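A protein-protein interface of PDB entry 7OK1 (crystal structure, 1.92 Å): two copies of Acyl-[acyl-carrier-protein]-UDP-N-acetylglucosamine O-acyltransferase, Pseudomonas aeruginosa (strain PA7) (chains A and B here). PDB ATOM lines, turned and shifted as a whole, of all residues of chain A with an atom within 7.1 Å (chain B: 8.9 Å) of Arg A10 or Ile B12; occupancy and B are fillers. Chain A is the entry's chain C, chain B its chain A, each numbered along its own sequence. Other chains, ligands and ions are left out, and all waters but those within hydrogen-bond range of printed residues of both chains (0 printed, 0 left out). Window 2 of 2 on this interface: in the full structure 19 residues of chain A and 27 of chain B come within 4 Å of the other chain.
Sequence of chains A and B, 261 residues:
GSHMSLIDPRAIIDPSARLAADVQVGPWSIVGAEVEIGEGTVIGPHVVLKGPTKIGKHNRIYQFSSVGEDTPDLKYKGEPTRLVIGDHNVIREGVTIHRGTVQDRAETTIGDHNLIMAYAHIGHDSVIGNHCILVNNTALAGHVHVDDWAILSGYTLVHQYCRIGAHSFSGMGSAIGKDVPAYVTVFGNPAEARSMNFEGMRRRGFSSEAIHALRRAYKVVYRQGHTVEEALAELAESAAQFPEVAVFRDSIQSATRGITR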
ATOM      1  N   ILE A   7      29.656   9.230   4.081  1.00  0.00           N
ATOM      2  CA  ILE A   7      28.891   8.201   3.360  1.00  0.00           C
ATOM      3  C   ILE A   7      27.459   8.665   3.498  1.00  0.00           C
ATOM      4  O   ILE A   7      26.927   8.638   4.615  1.00  0.00           O
ATOM      5  CB  ILE A   7      29.024   6.771   3.991  1.00  0.00           C
ATOM      6  CG1 ILE A   7      30.493   6.278   4.122  1.00  0.00           C
ATOM      7  CG2 ILE A   7      28.155   5.750   3.242  1.00  0.00           C
ATOM      8  CD1 ILE A   7      31.347   6.224   2.852  1.00  0.00           C
ATOM      9  N   ASP A   8      26.830   9.104   2.389  1.00  0.00           N
ATOM     10  CA  ASP A   8      25.445   9.570   2.420  1.00  0.00           C
ATOM     11  C   ASP A   8      24.537   8.433   2.946  1.00  0.00           C
ATOM     12  O   ASP A   8      24.735   7.282   2.558  1.00  0.00           O
ATOM     13  CB  ASP A   8      24.998  10.019   1.026  1.00  0.00           C
ATOM     14  CG  ASP A   8      23.652  10.698   1.022  1.00  0.00           C
ATOM     15  OD1 ASP A   8      22.631   9.987   1.013  1.00  0.00           O
ATOM     16  OD2 ASP A   8      23.616  11.937   1.048  1.00  0.00           O
ATOM     17  N   PRO A   9      23.537   8.717   3.813  1.00  0.00           N
ATOM     18  CA  PRO A   9      22.681   7.624   4.316  1.00  0.00           C
ATOM     19  C   PRO A   9      21.847   6.895   3.240  1.00  0.00           C
ATOM     20  O   PRO A   9      21.357   5.785   3.496  1.00  0.00           O
ATOM     21  CB  PRO A   9      21.818   8.299   5.403  1.00  0.00           C
ATOM     22  CG  PRO A   9      21.859   9.738   5.088  1.00  0.00           C
ATOM     23  CD  PRO A   9      23.162  10.018   4.405  1.00  0.00           C
ATOM     24  N   ARG A  10      21.702   7.500   2.042  1.00  0.00           N
ATOM     25  CA  ARG A  10      20.974   6.893   0.918  1.00  0.00           C
ATOM     26  C   ARG A  10      21.845   5.961   0.047  1.00  0.00           C
ATOM     27  O   ARG A  10      21.318   5.295  -0.847  1.00  0.00           O
ATOM     28  CB  ARG A  10      20.266   7.953   0.059  1.00  0.00           C
ATOM     29  CG  ARG A  10      19.191   8.724   0.823  1.00  0.00           C
ATOM     30  CD  ARG A  10      18.985  10.102   0.251  1.00  0.00           C
ATOM     31  NE  ARG A  10      20.103  10.997   0.557  1.00  0.00           N
ATOM     32  CZ  ARG A  10      19.990  12.312   0.699  1.00  0.00           C
ATOM     33  NH1 ARG A  10      18.803  12.898   0.598  1.00  0.00           N
ATOM     34  NH2 ARG A  10      21.059  13.050   0.972  1.00  0.00           N
ATOM     35  N   ALA A  11      23.155   5.895   0.326  1.00  0.00           N
ATOM     36  CA  ALA A  11      24.087   5.010  -0.382  1.00  0.00           C
ATOM     37  C   ALA A  11      23.967   3.584   0.168  1.00  0.00           C
ATOM     38  O   ALA A  11      23.493   3.385   1.298  1.00  0.00           O
ATOM     39  CB  ALA A  11      25.519   5.508  -0.198  1.00  0.00           C
ATOM     40  N   ILE A  12      24.390   2.592  -0.637  1.00  0.00           N
ATOM     41  CA  ILE A  12      24.378   1.193  -0.240  1.00  0.00           C
ATOM     42  C   ILE A  12      25.817   0.733  -0.195  1.00  0.00           C
ATOM     43  O   ILE A  12      26.476   0.709  -1.237  1.00  0.00           O
ATOM     44  CB  ILE A  12      23.522   0.288  -1.167  1.00  0.00           C
ATOM     45  CG1 ILE A  12      22.050   0.756  -1.224  1.00  0.00           C
ATOM     46  CG2 ILE A  12      23.658  -1.189  -0.715  1.00  0.00           C
ATOM     47  CD1 ILE A  12      21.120  -0.073  -2.165  1.00  0.00           C
ATOM     48  N   VAL A  25      30.874   9.023  -0.243  1.00  0.00           N
ATOM     49  CA  VAL A  25      29.955   8.299  -1.156  1.00  0.00           C
ATOM     50  C   VAL A  25      28.634   9.059  -1.230  1.00  0.00           C
ATOM     51  O   VAL A  25      27.978   9.279  -0.201  1.00  0.00           O
ATOM     52  CB  VAL A  25      29.759   6.801  -0.811  1.00  0.00           C
ATOM     53  CG1 VAL A  25      28.816   6.146  -1.815  1.00  0.00           C
ATOM     54  CG2 VAL A  25      31.088   6.053  -0.796  1.00  0.00           C
ATOM     55  N   GLY A  26      28.287   9.493  -2.435  1.00  0.00           N
ATOM     56  CA  GLY A  26      27.084  10.277  -2.674  1.00  0.00           C
ATOM     57  C   GLY A  26      25.801   9.482  -2.559  1.00  0.00           C
ATOM     58  O   GLY A  26      25.820   8.246  -2.445  1.00  0.00           O
ATOM     59  N   PRO A  27      24.649  10.182  -2.588  1.00  0.00           N
ATOM     60  CA  PRO A  27      23.368   9.476  -2.473  1.00  0.00           C
ATOM     61  C   PRO A  27      23.100   8.540  -3.645  1.00  0.00           C
ATOM     62  O   PRO A  27      23.510   8.822  -4.785  1.00  0.00           O
ATOM     63  CB  PRO A  27      22.346  10.621  -2.445  1.00  0.00           C
ATOM     64  CG  PRO A  27      23.021  11.747  -3.183  1.00  0.00           C
ATOM     65  CD  PRO A  27      24.443  11.643  -2.715  1.00  0.00           C
ATOM     66  N   TRP A  28      22.382   7.435  -3.357  1.00  0.00           N
ATOM     67  CA  TRP A  28      21.909   6.427  -4.309  1.00  0.00           C
ATOM     68  C   TRP A  28      23.059   5.745  -5.060  1.00  0.00           C
ATOM     69  O   TRP A  28      22.907   5.296  -6.192  1.00  0.00           O
ATOM     70  CB  TRP A  28      20.847   7.021  -5.256  1.00  0.00           C
ATOM     71  CG  TRP A  28      19.909   7.978  -4.590  1.00  0.00           C
ATOM     72  CD1 TRP A  28      18.985   7.687  -3.624  1.00  0.00           C
ATOM     73  CD2 TRP A  28      19.866   9.403  -4.774  1.00  0.00           C
ATOM     74  NE1 TRP A  28      18.329   8.835  -3.237  1.00  0.00           N
ATOM     75  CE2 TRP A  28      18.849   9.903  -3.925  1.00  0.00           C
ATOM     76  CE3 TRP A  28      20.544  10.302  -5.629  1.00  0.00           C
ATOM     77  CZ2 TRP A  28      18.523  11.266  -3.869  1.00  0.00           C
ATOM     78  CZ3 TRP A  28      20.199  11.648  -5.594  1.00  0.00           C
ATOM     79  CH2 TRP A  28      19.206  12.117  -4.716  1.00  0.00           C
ATOM     80  N   SER A  29      24.213   5.671  -4.406  1.00  0.00           N
ATOM     81  CA  SER A  29      25.376   5.020  -4.969  1.00  0.00           C
ATOM     82  C   SER A  29      25.493   3.627  -4.365  1.00  0.00           C
ATOM     83  O   SER A  29      25.068   3.406  -3.234  1.00  0.00           O
ATOM     84  CB  SER A  29      26.627   5.838  -4.699  1.00  0.00           C
ATOM     85  OG  SER A  29      26.681   6.896  -5.642  1.00  0.00           O
ATOM     86  N   ILE A  30      26.016   2.680  -5.139  1.00  0.00           N
ATOM     87  CA  ILE A  30      26.162   1.319  -4.664  1.00  0.00           C
ATOM     88  C   ILE A  30      27.620   0.959  -4.652  1.00  0.00           C
ATOM     89  O   ILE A  30      28.274   0.997  -5.696  1.00  0.00           O
ATOM     90  CB  ILE A  30      25.325   0.306  -5.486  1.00  0.00           C
ATOM     91  CG1 ILE A  30      23.825   0.689  -5.480  1.00  0.00           C
ATOM     92  CG2 ILE A  30      25.560  -1.121  -4.933  1.00  0.00           C
ATOM     93  CD1 ILE A  30      22.871  -0.184  -6.435  1.00  0.00           C
ATOM     94  N   PRO A  45      27.147  10.853  -6.770  1.00  0.00           N
ATOM     95  CA  PRO A  45      25.846  10.181  -6.599  1.00  0.00           C
ATOM     96  C   PRO A  45      25.575   9.243  -7.780  1.00  0.00           C
ATOM     97  O   PRO A  45      26.257   9.339  -8.794  1.00  0.00           O
ATOM     98  CB  PRO A  45      24.858  11.338  -6.579  1.00  0.00           C
ATOM     99  CG  PRO A  45      25.523  12.422  -7.490  1.00  0.00           C
ATOM    100  CD  PRO A  45      27.008  12.206  -7.374  1.00  0.00           C
ATOM    101  N   ILE B   7       7.686  19.148  -6.424  1.00  0.00           N
ATOM    102  CA  ILE B   7       9.041  18.753  -6.053  1.00  0.00           C
ATOM    103  C   ILE B   7       8.892  17.412  -5.311  1.00  0.00           C
ATOM    104  O   ILE B   7       8.279  17.354  -4.232  1.00  0.00           O
ATOM    105  CB  ILE B   7       9.792  19.780  -5.151  1.00  0.00           C
ATOM    106  CG1 ILE B   7       9.877  21.227  -5.775  1.00  0.00           C
ATOM    107  CG2 ILE B   7      11.175  19.235  -4.747  1.00  0.00           C
ATOM    108  CD1 ILE B   7      10.395  21.384  -7.138  1.00  0.00           C
ATOM    109  N   ASP B   8       9.438  16.344  -5.895  1.00  0.00           N
ATOM    110  CA  ASP B   8       9.371  15.029  -5.280  1.00  0.00           C
ATOM    111  C   ASP B   8      10.140  15.059  -3.948  1.00  0.00           C
ATOM    112  O   ASP B   8      11.203  15.681  -3.891  1.00  0.00           O
ATOM    113  CB  ASP B   8       9.935  13.959  -6.235  1.00  0.00           C
ATOM    114  CG  ASP B   8       9.694  12.555  -5.739  1.00  0.00           C
ATOM    115  OD1 ASP B   8      10.464  12.091  -4.858  1.00  0.00           O
ATOM    116  OD2 ASP B   8       8.717  11.925  -6.199  1.00  0.00           O
ATOM    117  N   PRO B   9       9.602  14.445  -2.858  1.00  0.00           N
ATOM    118  CA  PRO B   9      10.334  14.457  -1.570  1.00  0.00           C
ATOM    119  C   PRO B   9      11.687  13.727  -1.593  1.00  0.00           C
ATOM    120  O   PRO B   9      12.495  13.944  -0.704  1.00  0.00           O
ATOM    121  CB  PRO B   9       9.343  13.817  -0.578  1.00  0.00           C
ATOM    122  CG  PRO B   9       8.446  12.980  -1.416  1.00  0.00           C
ATOM    123  CD  PRO B   9       8.335  13.681  -2.755  1.00  0.00           C
ATOM    124  N   ARG B  10      11.950  12.896  -2.617  1.00  0.00           N
ATOM    125  CA  ARG B  10      13.226  12.160  -2.742  1.00  0.00           C
ATOM    126  C   ARG B  10      14.288  12.971  -3.500  1.00  0.00           C
ATOM    127  O   ARG B  10      15.448  12.553  -3.566  1.00  0.00           O
ATOM    128  CB  ARG B  10      13.009  10.775  -3.386  1.00  0.00           C
ATOM    129  CG  ARG B  10      12.217   9.828  -2.463  1.00  0.00           C
ATOM    130  CD  ARG B  10      11.483   8.754  -3.253  1.00  0.00           C
ATOM    131  NE  ARG B  10      10.340   9.293  -4.003  1.00  0.00           N
ATOM    132  CZ  ARG B  10       9.298   8.562  -4.391  1.00  0.00           C
ATOM    133  NH1 ARG B  10       9.242   7.269  -4.106  1.00  0.00           N
ATOM    134  NH2 ARG B  10       8.303   9.119  -5.065  1.00  0.00           N
ATOM    135  N   ALA B  11      13.884  14.126  -4.067  1.00  0.00           N
ATOM    136  CA  ALA B  11      14.772  15.042  -4.792  1.00  0.00           C
ATOM    137  C   ALA B  11      15.549  15.907  -3.781  1.00  0.00           C
ATOM    138  O   ALA B  11      15.065  16.125  -2.668  1.00  0.00           O
ATOM    139  CB  ALA B  11      13.951  15.938  -5.712  1.00  0.00           C
ATOM    140  N   ILE B  12      16.755  16.380  -4.157  1.00  0.00           N
ATOM    141  CA  ILE B  12      17.594  17.239  -3.302  1.00  0.00           C
ATOM    142  C   ILE B  12      17.635  18.642  -3.936  1.00  0.00           C
ATOM    143  O   ILE B  12      18.071  18.796  -5.081  1.00  0.00           O
ATOM    144  CB  ILE B  12      19.016  16.638  -3.056  1.00  0.00           C
ATOM    145  CG1 ILE B  12      18.936  15.275  -2.303  1.00  0.00           C
ATOM    146  CG2 ILE B  12      19.924  17.631  -2.263  1.00  0.00           C
ATOM    147  CD1 ILE B  12      20.270  14.450  -2.279  1.00  0.00           C
ATOM    148  N   ILE B  13      17.100  19.642  -3.222  1.00  0.00           N
ATOM    149  CA  ILE B  13      17.090  21.024  -3.685  1.00  0.00           C
ATOM    150  C   ILE B  13      18.036  21.803  -2.796  1.00  0.00           C
ATOM    151  O   ILE B  13      17.784  21.921  -1.598  1.00  0.00           O
ATOM    152  CB  ILE B  13      15.664  21.665  -3.713  1.00  0.00           C
ATOM    153  CG1 ILE B  13      14.572  20.722  -4.337  1.00  0.00           C
ATOM    154  CG2 ILE B  13      15.687  23.046  -4.406  1.00  0.00           C
ATOM    155  CD1 ILE B  13      14.781  20.219  -5.768  1.00  0.00           C
ATOM    156  N   ASP B  14      19.137  22.315  -3.359  1.00  0.00           N
ATOM    157  CA  ASP B  14      20.068  23.100  -2.557  1.00  0.00           C
ATOM    158  C   ASP B  14      19.350  24.400  -2.102  1.00  0.00           C
ATOM    159  O   ASP B  14      18.598  24.965  -2.900  1.00  0.00           O
ATOM    160  CB  ASP B  14      21.310  23.446  -3.375  1.00  0.00           C
ATOM    161  CG  ASP B  14      22.410  24.031  -2.526  1.00  0.00           C
ATOM    162  OD1 ASP B  14      22.428  25.292  -2.345  1.00  0.00           O
ATOM    163  OD2 ASP B  14      23.227  23.249  -2.003  1.00  0.00           O
ATOM    164  N   PRO B  15      19.546  24.862  -0.831  1.00  0.00           N
ATOM    165  CA  PRO B  15      18.869  26.111  -0.380  1.00  0.00           C
ATOM    166  C   PRO B  15      19.212  27.393  -1.179  1.00  0.00           C
ATOM    167  O   PRO B  15      18.402  28.326  -1.193  1.00  0.00           O
ATOM    168  CB  PRO B  15      19.255  26.222   1.098  1.00  0.00           C
ATOM    169  CG  PRO B  15      20.418  25.321   1.293  1.00  0.00           C
ATOM    170  CD  PRO B  15      20.367  24.255   0.250  1.00  0.00           C
ATOM    171  N   ALA B  17      19.451  27.445  -4.535  1.00  0.00           N
ATOM    172  CA  ALA B  17      18.763  27.298  -5.817  1.00  0.00           C
ATOM    173  C   ALA B  17      17.503  28.163  -5.819  1.00  0.00           C
ATOM    174  O   ALA B  17      16.861  28.275  -4.778  1.00  0.00           O
ATOM    175  CB  ALA B  17      18.411  25.826  -6.058  1.00  0.00           C
ATOM    176  N   LEU B  19      13.880  28.705  -7.693  1.00  0.00           N
ATOM    177  CA  LEU B  19      12.915  28.019  -8.543  1.00  0.00           C
ATOM    178  C   LEU B  19      11.602  28.795  -8.669  1.00  0.00           C
ATOM    179  O   LEU B  19      11.163  29.427  -7.696  1.00  0.00           O
ATOM    180  CB  LEU B  19      12.633  26.623  -7.932  1.00  0.00           C
ATOM    181  CG  LEU B  19      13.556  25.425  -8.349  1.00  0.00           C
ATOM    182  CD1 LEU B  19      14.980  25.558  -7.792  1.00  0.00           C
ATOM    183  CD2 LEU B  19      13.005  24.125  -7.836  1.00  0.00           C
ATOM    184  N   VAL B  25      10.152  18.576 -10.155  1.00  0.00           N
ATOM    185  CA  VAL B  25      11.437  17.882  -9.970  1.00  0.00           C
ATOM    186  C   VAL B  25      11.160  16.438  -9.599  1.00  0.00           C
ATOM    187  O   VAL B  25      10.446  16.178  -8.626  1.00  0.00           O
ATOM    188  CB  VAL B  25      12.446  18.597  -9.020  1.00  0.00           C
ATOM    189  CG1 VAL B  25      13.751  17.819  -8.947  1.00  0.00           C
ATOM    190  CG2 VAL B  25      12.715  20.034  -9.478  1.00  0.00           C
ATOM    191  N   GLY B  26      11.671  15.521 -10.414  1.00  0.00           N
ATOM    192  CA  GLY B  26      11.455  14.098 -10.213  1.00  0.00           C
ATOM    193  C   GLY B  26      12.240  13.492  -9.065  1.00  0.00           C
ATOM    194  O   GLY B  26      13.149  14.133  -8.516  1.00  0.00           O
ATOM    195  N   PRO B  27      11.893  12.237  -8.656  1.00  0.00           N
ATOM    196  CA  PRO B  27      12.635  11.596  -7.546  1.00  0.00           C
ATOM    197  C   PRO B  27      14.114  11.363  -7.867  1.00  0.00           C
ATOM    198  O   PRO B  27      14.468  11.040  -9.003  1.00  0.00           O
ATOM    199  CB  PRO B  27      11.897  10.257  -7.348  1.00  0.00           C
ATOM    200  CG  PRO B  27      11.272   9.974  -8.688  1.00  0.00           C
ATOM    201  CD  PRO B  27      10.861  11.334  -9.214  1.00  0.00           C
ATOM    202  N   TRP B  28      14.970  11.501  -6.852  1.00  0.00           N
ATOM    203  CA  TRP B  28      16.420  11.246  -6.909  1.00  0.00           C
ATOM    204  C   TRP B  28      17.147  12.204  -7.865  1.00  0.00           C
ATOM    205  O   TRP B  28      18.209  11.895  -8.408  1.00  0.00           O
ATOM    206  CB  TRP B  28      16.750   9.755  -7.199  1.00  0.00           C
ATOM    207  CG  TRP B  28      15.808   8.759  -6.576  1.00  0.00           C
ATOM    208  CD1 TRP B  28      15.670   8.475  -5.248  1.00  0.00           C
ATOM    209  CD2 TRP B  28      14.862   7.916  -7.268  1.00  0.00           C
ATOM    210  NE1 TRP B  28      14.696   7.514  -5.066  1.00  0.00           N
ATOM    211  CE2 TRP B  28      14.206   7.132  -6.292  1.00  0.00           C
ATOM    212  CE3 TRP B  28      14.503   7.753  -8.621  1.00  0.00           C
ATOM    213  CZ2 TRP B  28      13.220   6.187  -6.627  1.00  0.00           C
ATOM    214  CZ3 TRP B  28      13.554   6.789  -8.956  1.00  0.00           C
ATOM    215  CH2 TRP B  28      12.919   6.024  -7.968  1.00  0.00           C
ATOM    216  N   SER B  29      16.578  13.404  -8.028  1.00  0.00           N
ATOM    217  CA  SER B  29      17.194  14.446  -8.821  1.00  0.00           C
ATOM    218  C   SER B  29      17.887  15.436  -7.882  1.00  0.00           C
ATOM    219  O   SER B  29      17.472  15.592  -6.731  1.00  0.00           O
ATOM    220  CB  SER B  29      16.178  15.122  -9.730  1.00  0.00           C
ATOM    221  OG  SER B  29      15.946  14.203 -10.780  1.00  0.00           O
ATOM    222  N   ILE B  30      18.990  16.029  -8.354  1.00  0.00           N
ATOM    223  CA  ILE B  30      19.777  16.981  -7.581  1.00  0.00           C
ATOM    224  C   ILE B  30      19.722  18.332  -8.254  1.00  0.00           C
ATOM    225  O   ILE B  30      20.117  18.448  -9.412  1.00  0.00           O
ATOM    226  CB  ILE B  30      21.235  16.473  -7.382  1.00  0.00           C
ATOM    227  CG1 ILE B  30      21.254  15.189  -6.529  1.00  0.00           C
ATOM    228  CG2 ILE B  30      22.127  17.586  -6.771  1.00  0.00           C
ATOM    229  CD1 ILE B  30      22.628  14.474  -6.373  1.00  0.00           C
ATOM    230  N   VAL B  31      19.199  19.346  -7.546  1.00  0.00           N
ATOM    231  CA  VAL B  31      19.173  20.733  -8.029  1.00  0.00           C
ATOM    232  C   VAL B  31      20.229  21.387  -7.138  1.00  0.00           C
ATOM    233  O   VAL B  31      19.960  21.724  -5.978  1.00  0.00           O
ATOM    234  CB  VAL B  31      17.768  21.407  -7.952  1.00  0.00           C
ATOM    235  CG1 VAL B  31      17.834  22.889  -8.306  1.00  0.00           C
ATOM    236  CG2 VAL B  31      16.776  20.700  -8.862  1.00  0.00           C
ATOM    237  N   GLY B  32      21.451  21.429  -7.656  1.00  0.00           N
ATOM    238  CA  GLY B  32      22.612  21.934  -6.934  1.00  0.00           C
ATOM    239  C   GLY B  32      22.623  23.417  -6.635  1.00  0.00           C
ATOM    240  O   GLY B  32      21.662  24.150  -6.927  1.00  0.00           O
ATOM    241  N   ALA B  33      23.716  23.852  -5.991  1.00  0.00           N
ATOM    242  CA  ALA B  33      23.908  25.238  -5.597  1.00  0.00           C
ATOM    243  C   ALA B  33      23.951  26.129  -6.818  1.00  0.00           C
ATOM    244  O   ALA B  33      24.451  25.723  -7.875  1.00  0.00           O
ATOM    245  CB  ALA B  33      25.183  25.402  -4.761  1.00  0.00           C
ATOM    246  N   VAL B  35      21.591  27.066  -8.867  1.00  0.00           N
ATOM    247  CA  VAL B  35      20.819  26.623 -10.040  1.00  0.00           C
ATOM    248  C   VAL B  35      19.525  27.409  -9.969  1.00  0.00           C
ATOM    249  O   VAL B  35      18.922  27.510  -8.905  1.00  0.00           O
ATOM    250  CB  VAL B  35      20.585  25.079 -10.134  1.00  0.00           C
ATOM    251  CG1 VAL B  35      19.590  24.717 -11.251  1.00  0.00           C
ATOM    252  CG2 VAL B  35      21.899  24.326 -10.346  1.00  0.00           C
ATOM    253  N   ILE B  37      15.785  27.775 -11.854  1.00  0.00           N
ATOM    254  CA  ILE B  37      14.858  27.093 -12.755  1.00  0.00           C
ATOM    255  C   ILE B  37      13.570  27.911 -12.941  1.00  0.00           C
ATOM    256  O   ILE B  37      12.889  28.232 -11.972  1.00  0.00           O
ATOM    257  CB  ILE B  37      14.579  25.598 -12.399  1.00  0.00           C
ATOM    258  CG1 ILE B  37      15.864  24.801 -12.052  1.00  0.00           C
ATOM    259  CG2 ILE B  37      13.842  24.919 -13.546  1.00  0.00           C
ATOM    260  CD1 ILE B  37      15.579  23.358 -11.470  1.00  0.00           C
ATOM    261  N   ILE B  43      11.808  18.718 -14.531  1.00  0.00           N
ATOM    262  CA  ILE B  43      13.054  17.988 -14.336  1.00  0.00           C
ATOM    263  C   ILE B  43      12.618  16.561 -14.059  1.00  0.00           C
ATOM    264  O   ILE B  43      11.786  16.352 -13.177  1.00  0.00           O
ATOM    265  CB  ILE B  43      13.916  18.594 -13.191  1.00  0.00           C
ATOM    266  CG1 ILE B  43      14.127  20.150 -13.348  1.00  0.00           C
ATOM    267  CG2 ILE B  43      15.233  17.839 -13.045  1.00  0.00           C
ATOM    268  CD1 ILE B  43      14.958  20.618 -14.621  1.00  0.00           C
ATOM    269  N   VAL B  47      18.277  13.226 -12.368  1.00  0.00           N
ATOM    270  CA  VAL B  47      18.930  14.307 -13.112  1.00  0.00           C
ATOM    271  C   VAL B  47      19.897  15.019 -12.169  1.00  0.00           C
ATOM    272  O   VAL B  47      19.565  15.221 -11.007  1.00  0.00           O
ATOM    273  CB  VAL B  47      17.874  15.276 -13.703  1.00  0.00           C
ATOM    274  CG1 VAL B  47      18.518  16.528 -14.319  1.00  0.00           C
ATOM    275  CG2 VAL B  47      16.984  14.568 -14.716  1.00  0.00           C
ATOM    276  N   VAL B  48      21.092  15.372 -12.655  1.00  0.00           N
ATOM    277  CA  VAL B  48      22.057  16.144 -11.876  1.00  0.00           C
ATOM    278  C   VAL B  48      22.148  17.537 -12.502  1.00  0.00           C
ATOM    279  O   VAL B  48      22.454  17.675 -13.698  1.00  0.00           O
ATOM    280  CB  VAL B  48      23.447  15.477 -11.689  1.00  0.00           C
ATOM    281  CG1 VAL B  48      24.383  16.365 -10.847  1.00  0.00           C
ATOM    282  CG2 VAL B  48      23.301  14.112 -11.029  1.00  0.00           C
ATOM    283  N   LEU B  49      21.815  18.563 -11.693  1.00  0.00           N
ATOM    284  CA  LEU B  49      21.931  19.959 -12.087  1.00  0.00           C
ATOM    285  C   LEU B  49      22.947  20.600 -11.206  1.00  0.00           C
ATOM    286  O   LEU B  49      22.838  20.509  -9.985  1.00  0.00           O
ATOM    287  CB  LEU B  49      20.599  20.720 -12.033  1.00  0.00           C
ATOM    288  CG  LEU B  49      19.427  20.133 -12.823  1.00  0.00           C
ATOM    289  CD1 LEU B  49      18.211  21.051 -12.671  1.00  0.00           C
ATOM    290  CD2 LEU B  49      19.783  19.942 -14.320  1.00  0.00           C
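Arg A10 touches one residue of chain B.
Ile B12 touches just these residues of chain A: Arg A10 (3.6 Å), Pro A27 (3.96 Å) and Trp A28 (3.5 Å).
Of the printed residues of chain B, Pro A45 touches Ile B30.
Printed residues of chain B within 4 Å of Trp A28: Arg B10 (3.3 Å), Ile B12 (3.5 Å), Trp B28 (3.4 Å) and Ile B30 (3.8 Å).
Of the printed residues of chain A, Trp B28 touches Trp A28 (3.4 Å).
Of the printed residues of chain A, Ile B30 touches Trp A28 and Pro A45.
Printed residues of chain A within 4 Å of Arg B10: Trp A28 (3.3 Å).
Pro B27 touches none of the printed residues of chain A.
The nearest residue of chain B that does not touch Arg A10 is Arg B10 (5.4 Å).
The nearest residue of chain A that does not touch Ile B12 is Asp A8 (5.3 Å).
The nearest printed residue of chain A that does not touch Trp B28 is Arg A10 (6.6 Å).
Arg A10 touches Ile B12.
CG of Pro A27 touches CD1 of Ile B12 (3.96 Å).
O of Arg B10 touches CZ2 of Trp A28, 3.3 Å away.
CD1 of Ile B12 touches CH2 of Trp A28 (3.5 Å).
CD1 of Trp B28 touches NE1 of Trp A28, 3.4 Å away.
CZ3 of Trp A28 touches CD1 of Ile B30, at 3.8 Å.
Pro A45 touches Ile B30.
Arg A10 touches Ile B12, but with the chains exchanged Ile A12 does not touch Arg B10 (13.1 Å).
Pro A27 touches Ile B12, but with the chains exchanged Ile A12 does not touch Pro B27 (14.6 Å).
Trp A28 touches Arg B10, but with the chains exchanged Arg A10 does not touch Trp B28 (6.6 Å).
Trp A28 touches Ile B12, but with the chains exchanged Ile A12 does not touch Trp B28 (10.4 Å).
Positions printed for both chains: 7, 8, 9, 10, 11, 12, 25, 26, 27, 28, 29 and 30.
Of the 7 pairs that touch across the chains among the printed residues, 1 has its exchanged pair printed and touching as well.
The backbone carbonyl oxygen (O) of Arg B10 lies within hydrogen-bond range of the backbone NH (N) of Trp B28 (3.5 Å).
The guanidinium group of Arg A10 lies within salt-bridge range of the side-chain carboxylate of Asp A8 (2.8 Å).
O of Arg A10 is in hydrogen-bond range of N of Trp A28 (3.5 Å).
The side-chain carboxylate (OD1) of Asp B8 is in salt-bridge range of the guanidinium group (NE) of Arg B10.
O of Ile B30 lies within hydrogen-bond range of N of Leu B49, 2.8 Å away.
The backbone NH (N) of Val B31 is in hydrogen-bond range of the backbone carbonyl oxygen (O) of Ile B12 (2.8 Å).
Of the 13 printed residues of chain A, 4 touch a printed residue of chain B.
Hydrophobic or aromatic side chains of chain A within 4 Å of the printed part of chain B: Pro A27, Trp A28 and Pro A45.
Of the 26 printed residues of chain B, 4 touch a printed residue of chain A.
Hydrophobic or aromatic side chains of chain B that line the printed part of chain A: Ile B12, Trp B28 and Ile B30.
Among the printed residues, 7 pairs touch across the chains.
Among the printed residues, no Asp or Glu carboxylate lies within 4 Å of a Lys or Arg side-chain nitrogen of the other chain.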
